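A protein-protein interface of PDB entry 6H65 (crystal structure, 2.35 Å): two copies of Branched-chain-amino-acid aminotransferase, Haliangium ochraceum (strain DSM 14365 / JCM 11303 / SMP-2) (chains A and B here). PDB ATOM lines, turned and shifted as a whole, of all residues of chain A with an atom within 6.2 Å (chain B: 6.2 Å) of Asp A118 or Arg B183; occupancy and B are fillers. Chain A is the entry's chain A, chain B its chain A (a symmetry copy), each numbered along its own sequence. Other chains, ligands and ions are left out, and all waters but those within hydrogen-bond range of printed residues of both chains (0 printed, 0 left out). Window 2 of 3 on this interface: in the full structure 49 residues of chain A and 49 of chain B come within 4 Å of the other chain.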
ATOM      1  N   ASN A 116     -12.510 -18.470  -6.169  1.00  0.00           N
ATOM      2  CA  ASN A 116     -11.973 -19.588  -5.431  1.00  0.00           C
ATOM      3  C   ASN A 116     -10.696 -19.224  -4.688  1.00  0.00           C
ATOM      4  O   ASN A 116      -9.804 -18.583  -5.227  1.00  0.00           O
ATOM      5  CB  ASN A 116     -11.489 -20.632  -6.414  1.00  0.00           C
ATOM      6  CG  ASN A 116     -12.465 -21.762  -6.491  1.00  0.00           C
ATOM      7  OD1 ASN A 116     -12.652 -22.446  -5.485  1.00  0.00           O
ATOM      8  ND2 ASN A 116     -13.003 -21.978  -7.684  1.00  0.00           N
ATOM      9  N   HIS A 117     -10.604 -19.736  -3.458  1.00  0.00           N
ATOM     10  CA  HIS A 117      -9.516 -19.452  -2.528  1.00  0.00           C
ATOM     11  C   HIS A 117      -8.638 -20.694  -2.378  1.00  0.00           C
ATOM     12  O   HIS A 117      -7.692 -20.680  -1.585  1.00  0.00           O
ATOM     13  CB  HIS A 117     -10.083 -18.980  -1.168  1.00  0.00           C
ATOM     14  CG  HIS A 117      -9.360 -17.828  -0.543  1.00  0.00           C
ATOM     15  ND1 HIS A 117      -9.924 -16.548  -0.472  1.00  0.00           N
ATOM     16  CD2 HIS A 117      -8.148 -17.762   0.070  1.00  0.00           C
ATOM     17  CE1 HIS A 117      -9.067 -15.738   0.132  1.00  0.00           C
ATOM     18  NE2 HIS A 117      -7.970 -16.459   0.479  1.00  0.00           N
ATOM     19  N   ASP A 118      -8.961 -21.755  -3.135  1.00  0.00           N
ATOM     20  CA  ASP A 118      -8.444 -23.093  -2.882  1.00  0.00           C
ATOM     21  C   ASP A 118      -8.160 -23.782  -4.212  1.00  0.00           C
ATOM     22  O   ASP A 118      -8.896 -23.601  -5.179  1.00  0.00           O
ATOM     23  CB  ASP A 118      -9.422 -23.906  -2.014  1.00  0.00           C
ATOM     24  CG  ASP A 118      -8.894 -25.249  -1.535  1.00  0.00           C
ATOM     25  OD1 ASP A 118      -8.583 -26.125  -2.378  1.00  0.00           O
ATOM     26  OD2 ASP A 118      -8.804 -25.419  -0.315  1.00  0.00           O
ATOM     27  N   PRO A 119      -7.100 -24.621  -4.295  1.00  0.00           N
ATOM     28  CA  PRO A 119      -6.832 -25.409  -5.506  1.00  0.00           C
ATOM     29  C   PRO A 119      -7.985 -26.312  -5.958  1.00  0.00           C
ATOM     30  O   PRO A 119      -8.163 -26.584  -7.138  1.00  0.00           O
ATOM     31  CB  PRO A 119      -5.641 -26.286  -5.108  1.00  0.00           C
ATOM     32  CG  PRO A 119      -4.975 -25.509  -3.991  1.00  0.00           C
ATOM     33  CD  PRO A 119      -6.110 -24.850  -3.231  1.00  0.00           C
ATOM     34  N   ASP A 120      -8.786 -26.797  -5.019  1.00  0.00           N
ATOM     35  CA  ASP A 120      -9.878 -27.710  -5.336  1.00  0.00           C
ATOM     36  C   ASP A 120     -11.126 -26.902  -5.735  1.00  0.00           C
ATOM     37  O   ASP A 120     -11.685 -26.165  -4.922  1.00  0.00           O
ATOM     38  CB  ASP A 120     -10.087 -28.624  -4.128  1.00  0.00           C
ATOM     39  CG  ASP A 120     -11.213 -29.627  -4.201  1.00  0.00           C
ATOM     40  OD1 ASP A 120     -11.860 -29.744  -5.310  1.00  0.00           O
ATOM     41  OD2 ASP A 120     -11.394 -30.309  -3.123  1.00  0.00           O
ATOM     42  N   PRO A 121     -11.638 -27.005  -6.987  1.00  0.00           N
ATOM     43  CA  PRO A 121     -12.737 -26.137  -7.434  1.00  0.00           C
ATOM     44  C   PRO A 121     -14.108 -26.527  -6.879  1.00  0.00           C
ATOM     45  O   PRO A 121     -15.094 -25.787  -6.994  1.00  0.00           O
ATOM     46  CB  PRO A 121     -12.723 -26.273  -8.944  1.00  0.00           C
ATOM     47  CG  PRO A 121     -12.119 -27.654  -9.177  1.00  0.00           C
ATOM     48  CD  PRO A 121     -11.164 -27.928  -8.028  1.00  0.00           C
ATOM     49  N   PHE A 123     -14.588 -27.165  -3.603  1.00  0.00           N
ATOM     50  CA  PHE A 123     -14.615 -26.825  -2.192  1.00  0.00           C
ATOM     51  C   PHE A 123     -15.091 -25.381  -2.085  1.00  0.00           C
ATOM     52  O   PHE A 123     -14.736 -24.543  -2.891  1.00  0.00           O
ATOM     53  CB  PHE A 123     -13.239 -27.109  -1.561  1.00  0.00           C
ATOM     54  CG  PHE A 123     -13.179 -27.063  -0.053  1.00  0.00           C
ATOM     55  CD1 PHE A 123     -13.582 -28.157   0.708  1.00  0.00           C
ATOM     56  CD2 PHE A 123     -12.703 -25.927   0.611  1.00  0.00           C
ATOM     57  CE1 PHE A 123     -13.520 -28.110   2.099  1.00  0.00           C
ATOM     58  CE2 PHE A 123     -12.670 -25.872   2.000  1.00  0.00           C
ATOM     59  CZ  PHE A 123     -13.070 -26.967   2.746  1.00  0.00           C
ATOM     60  N   PRO A 124     -15.920 -25.008  -1.093  1.00  0.00           N
ATOM     61  CA  PRO A 124     -16.473 -23.654  -1.030  1.00  0.00           C
ATOM     62  C   PRO A 124     -15.381 -22.644  -0.676  1.00  0.00           C
ATOM     63  O   PRO A 124     -14.374 -23.011  -0.068  1.00  0.00           O
ATOM     64  CB  PRO A 124     -17.495 -23.811   0.107  1.00  0.00           C
ATOM     65  CG  PRO A 124     -16.879 -24.798   1.032  1.00  0.00           C
ATOM     66  CD  PRO A 124     -16.314 -25.829   0.067  1.00  0.00           C
ATOM     67  N   THR A 125     -15.570 -21.386  -1.093  1.00  0.00           N
ATOM     68  CA  THR A 125     -14.598 -20.368  -0.753  1.00  0.00           C
ATOM     69  C   THR A 125     -15.161 -19.529   0.393  1.00  0.00           C
ATOM     70  O   THR A 125     -16.376 -19.516   0.620  1.00  0.00           O
ATOM     71  CB  THR A 125     -14.591 -19.203  -1.745  1.00  0.00           C
ATOM     72  OG1 THR A 125     -15.460 -19.302  -2.871  1.00  0.00           O
ATOM     73  CG2 THR A 125     -13.213 -18.662  -2.023  1.00  0.00           C
ATOM     74  N   ALA B 178     -20.324 -33.786  -1.579  1.00  0.00           N
ATOM     75  CA  ALA B 178     -19.505 -34.956  -1.332  1.00  0.00           C
ATOM     76  C   ALA B 178     -18.046 -34.539  -1.121  1.00  0.00           C
ATOM     77  O   ALA B 178     -17.402 -34.998  -0.174  1.00  0.00           O
ATOM     78  CB  ALA B 178     -19.697 -35.958  -2.444  1.00  0.00           C
ATOM     79  N   GLN B 179     -17.575 -33.566  -1.906  1.00  0.00           N
ATOM     80  CA  GLN B 179     -16.161 -33.218  -1.880  1.00  0.00           C
ATOM     81  C   GLN B 179     -15.824 -32.395  -0.639  1.00  0.00           C
ATOM     82  O   GLN B 179     -14.749 -32.557  -0.037  1.00  0.00           O
ATOM     83  CB  GLN B 179     -15.764 -32.426  -3.120  1.00  0.00           C
ATOM     84  CG  GLN B 179     -14.266 -32.112  -3.202  1.00  0.00           C
ATOM     85  CD  GLN B 179     -13.367 -33.328  -3.345  1.00  0.00           C
ATOM     86  OE1 GLN B 179     -13.774 -34.437  -3.654  1.00  0.00           O
ATOM     87  NE2 GLN B 179     -12.089 -33.151  -3.079  1.00  0.00           N
ATOM     88  N   THR B 180     -16.750 -31.511  -0.256  1.00  0.00           N
ATOM     89  CA  THR B 180     -16.551 -30.726   0.948  1.00  0.00           C
ATOM     90  C   THR B 180     -16.453 -31.677   2.137  1.00  0.00           C
ATOM     91  O   THR B 180     -15.529 -31.585   2.930  1.00  0.00           O
ATOM     92  CB  THR B 180     -17.651 -29.670   1.072  1.00  0.00           C
ATOM     93  OG1 THR B 180     -17.596 -28.935  -0.139  1.00  0.00           O
ATOM     94  CG2 THR B 180     -17.462 -28.749   2.246  1.00  0.00           C
ATOM     95  N   GLU B 181     -17.368 -32.645   2.191  1.00  0.00           N
ATOM     96  CA  GLU B 181     -17.370 -33.528   3.332  1.00  0.00           C
ATOM     97  C   GLU B 181     -16.058 -34.313   3.401  1.00  0.00           C
ATOM     98  O   GLU B 181     -15.506 -34.491   4.490  1.00  0.00           O
ATOM     99  CB  GLU B 181     -18.493 -34.545   3.186  1.00  0.00           C
ATOM    100  CG  GLU B 181     -18.389 -35.606   4.272  1.00  0.00           C
ATOM    101  CD  GLU B 181     -19.608 -36.513   4.377  1.00  0.00           C
ATOM    102  OE1 GLU B 181     -20.645 -36.033   4.965  1.00  0.00           O
ATOM    103  OE2 GLU B 181     -19.546 -37.677   3.789  1.00  0.00           O
ATOM    104  N   ALA B 182     -15.612 -34.842   2.242  1.00  0.00           N
ATOM    105  CA  ALA B 182     -14.354 -35.557   2.183  1.00  0.00           C
ATOM    106  C   ALA B 182     -13.217 -34.721   2.787  1.00  0.00           C
ATOM    107  O   ALA B 182     -12.466 -35.182   3.658  1.00  0.00           O
ATOM    108  CB  ALA B 182     -14.075 -35.987   0.756  1.00  0.00           C
ATOM    109  N   ARG B 183     -13.103 -33.473   2.348  1.00  0.00           N
ATOM    110  CA  ARG B 183     -11.977 -32.669   2.780  1.00  0.00           C
ATOM    111  C   ARG B 183     -12.135 -32.352   4.259  1.00  0.00           C
ATOM    112  O   ARG B 183     -11.147 -32.346   4.998  1.00  0.00           O
ATOM    113  CB  ARG B 183     -11.867 -31.360   1.989  1.00  0.00           C
ATOM    114  CG  ARG B 183     -11.635 -31.596   0.491  1.00  0.00           C
ATOM    115  CD  ARG B 183     -10.258 -32.091   0.049  1.00  0.00           C
ATOM    116  NE  ARG B 183      -9.194 -31.222   0.507  1.00  0.00           N
ATOM    117  CZ  ARG B 183      -9.012 -29.931   0.168  1.00  0.00           C
ATOM    118  NH1 ARG B 183      -9.644 -29.446  -0.884  1.00  0.00           N
ATOM    119  NH2 ARG B 183      -8.268 -29.119   0.916  1.00  0.00           N
ATOM    120  N   VAL B 184     -13.375 -32.087   4.690  1.00  0.00           N
ATOM    121  CA  VAL B 184     -13.589 -31.766   6.091  1.00  0.00           C
ATOM    122  C   VAL B 184     -13.112 -32.957   6.933  1.00  0.00           C
ATOM    123  O   VAL B 184     -12.586 -32.792   8.023  1.00  0.00           O
ATOM    124  CB  VAL B 184     -15.050 -31.327   6.375  1.00  0.00           C
ATOM    125  CG1 VAL B 184     -15.436 -31.462   7.838  1.00  0.00           C
ATOM    126  CG2 VAL B 184     -15.327 -29.905   5.899  1.00  0.00           C
ATOM    127  N   ASN B 185     -13.252 -34.175   6.407  1.00  0.00           N
ATOM    128  CA  ASN B 185     -12.932 -35.349   7.206  1.00  0.00           C
ATOM    129  C   ASN B 185     -11.488 -35.815   6.972  1.00  0.00           C
ATOM    130  O   ASN B 185     -11.147 -36.900   7.395  1.00  0.00           O
ATOM    131  CB  ASN B 185     -13.963 -36.442   6.878  1.00  0.00           C
ATOM    132  CG  ASN B 185     -15.315 -36.180   7.506  1.00  0.00           C
ATOM    133  OD1 ASN B 185     -15.437 -35.348   8.387  1.00  0.00           O
ATOM    134  ND2 ASN B 185     -16.332 -36.890   7.052  1.00  0.00           N
ATOM    135  N   GLY B 186     -10.654 -35.069   6.253  1.00  0.00           N
ATOM    136  CA  GLY B 186      -9.250 -35.456   6.133  1.00  0.00           C
ATOM    137  C   GLY B 186      -8.912 -36.382   4.943  1.00  0.00           C
ATOM    138  O   GLY B 186      -7.899 -37.058   4.983  1.00  0.00           O
ATOM    139  N   TYR B 187      -9.729 -36.397   3.884  1.00  0.00           N
ATOM    140  CA  TYR B 187      -9.507 -37.258   2.722  1.00  0.00           C
ATOM    141  C   TYR B 187      -9.352 -36.347   1.502  1.00  0.00           C
ATOM    142  O   TYR B 187      -9.795 -35.187   1.536  1.00  0.00           O
ATOM    143  CB  TYR B 187     -10.711 -38.181   2.478  1.00  0.00           C
ATOM    144  CG  TYR B 187     -10.988 -39.199   3.554  1.00  0.00           C
ATOM    145  CD1 TYR B 187     -10.303 -40.399   3.574  1.00  0.00           C
ATOM    146  CD2 TYR B 187     -11.886 -38.955   4.586  1.00  0.00           C
ATOM    147  CE1 TYR B 187     -10.491 -41.344   4.576  1.00  0.00           C
ATOM    148  CE2 TYR B 187     -12.122 -39.893   5.590  1.00  0.00           C
ATOM    149  CZ  TYR B 187     -11.416 -41.098   5.579  1.00  0.00           C
ATOM    150  OH  TYR B 187     -11.619 -42.049   6.544  1.00  0.00           O
ATOM    151  N   HIS B 188      -8.712 -36.843   0.434  1.00  0.00           N
ATOM    152  CA  HIS B 188      -8.580 -36.090  -0.809  1.00  0.00           C
ATOM    153  C   HIS B 188      -9.900 -36.100  -1.568  1.00  0.00           C
ATOM    154  O   HIS B 188     -10.211 -35.137  -2.244  1.00  0.00           O
ATOM    155  CB  HIS B 188      -7.433 -36.617  -1.689  1.00  0.00           C
ATOM    156  CG  HIS B 188      -6.083 -36.482  -1.053  1.00  0.00           C
ATOM    157  ND1 HIS B 188      -5.518 -37.481  -0.238  1.00  0.00           N
ATOM    158  CD2 HIS B 188      -5.176 -35.485  -1.088  1.00  0.00           C
ATOM    159  CE1 HIS B 188      -4.324 -37.091   0.195  1.00  0.00           C
ATOM    160  NE2 HIS B 188      -4.103 -35.875  -0.327  1.00  0.00           N
ATOM    161  N   THR B 189     -10.672 -37.193  -1.514  1.00  0.00           N
ATOM    162  CA  THR B 189     -11.943 -37.171  -2.226  1.00  0.00           C
ATOM    163  C   THR B 189     -12.789 -38.320  -1.698  1.00  0.00           C
ATOM    164  O   THR B 189     -12.397 -39.010  -0.754  1.00  0.00           O
ATOM    165  CB  THR B 189     -11.747 -37.193  -3.747  1.00  0.00           C
ATOM    166  OG1 THR B 189     -12.964 -36.852  -4.418  1.00  0.00           O
ATOM    167  CG2 THR B 189     -11.321 -38.538  -4.283  1.00  0.00           C
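Printed residues of chain A that touch a printed residue of chain B: Asp A118, Asp A120, Phe A123 and Pro A124.
Among the printed residues, Asp or Glu carboxylates within 4 Å of a Lys or Arg side-chain nitrogen of the other chain: Asp A118 with Arg B183 and Asp A120 with Arg B183.
The guanidinium group (NH1) of Arg B183 lies within salt-bridge range of the side-chain carboxylate (OD2) of Asp A120.
The side-chain amide nitrogen (NE2) of Gln B179 is in hydrogen-bond range of the side-chain carboxylate (OD2) of Asp A120, at 2.9 Å.
OD1 of Asp A118 lies within salt-bridge range of NH1 of Arg B183, 3.8 Å away.
The backbone NH of Asp A120 sits at hydrogen-bond distance from the side-chain carboxylate of Asp A118, 2.7 Å away.
NE2 of Gln B179 sits at hydrogen-bond distance from O of His B188 (2.9 Å).
OE1 of Gln B179 lies within hydrogen-bond range of OG1 of Thr B189 (2.7 Å).
Thr B180 touches Phe A123 (CA to CD1, 3.9 Å).
Phe A123 touches Arg B183.
Pro A124 touches Thr B180.
Of chain B, only Arg B183 (3.8 Å) comes within 4 Å of Asp A118.
Of the printed residues of chain B, Asp A120 touches Gln B179 (2.9 Å) and Arg B183 (3.0 Å).
Of the printed residues of chain B, Phe A123 touches Thr B180 and Arg B183.
Of the printed residues of chain B, Pro A124 touches Thr B180.
Printed residues of chain A within 4 Å of Gln B179: Asp A120.
Printed residues of chain A within 4 Å of Thr B180: Phe A123 (3.9 Å) and Pro A124 (3.4 Å).
Of chain A, only Asp A118 (3.8 Å), Asp A120 (3.0 Å) and Phe A123 (3.6 Å) come within 4 Å of Arg B183.
Val B184 touches none of the printed residues of chain A.
Asn B185 touches none of the printed residues of chain A.
The nearest printed residue of chain B that does not touch Asp A118 is Gln B179 (7.9 Å).
The nearest printed residue of chain A that does not touch Arg B183 is Pro A119 (6.2 Å).
No position is printed for both chains.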
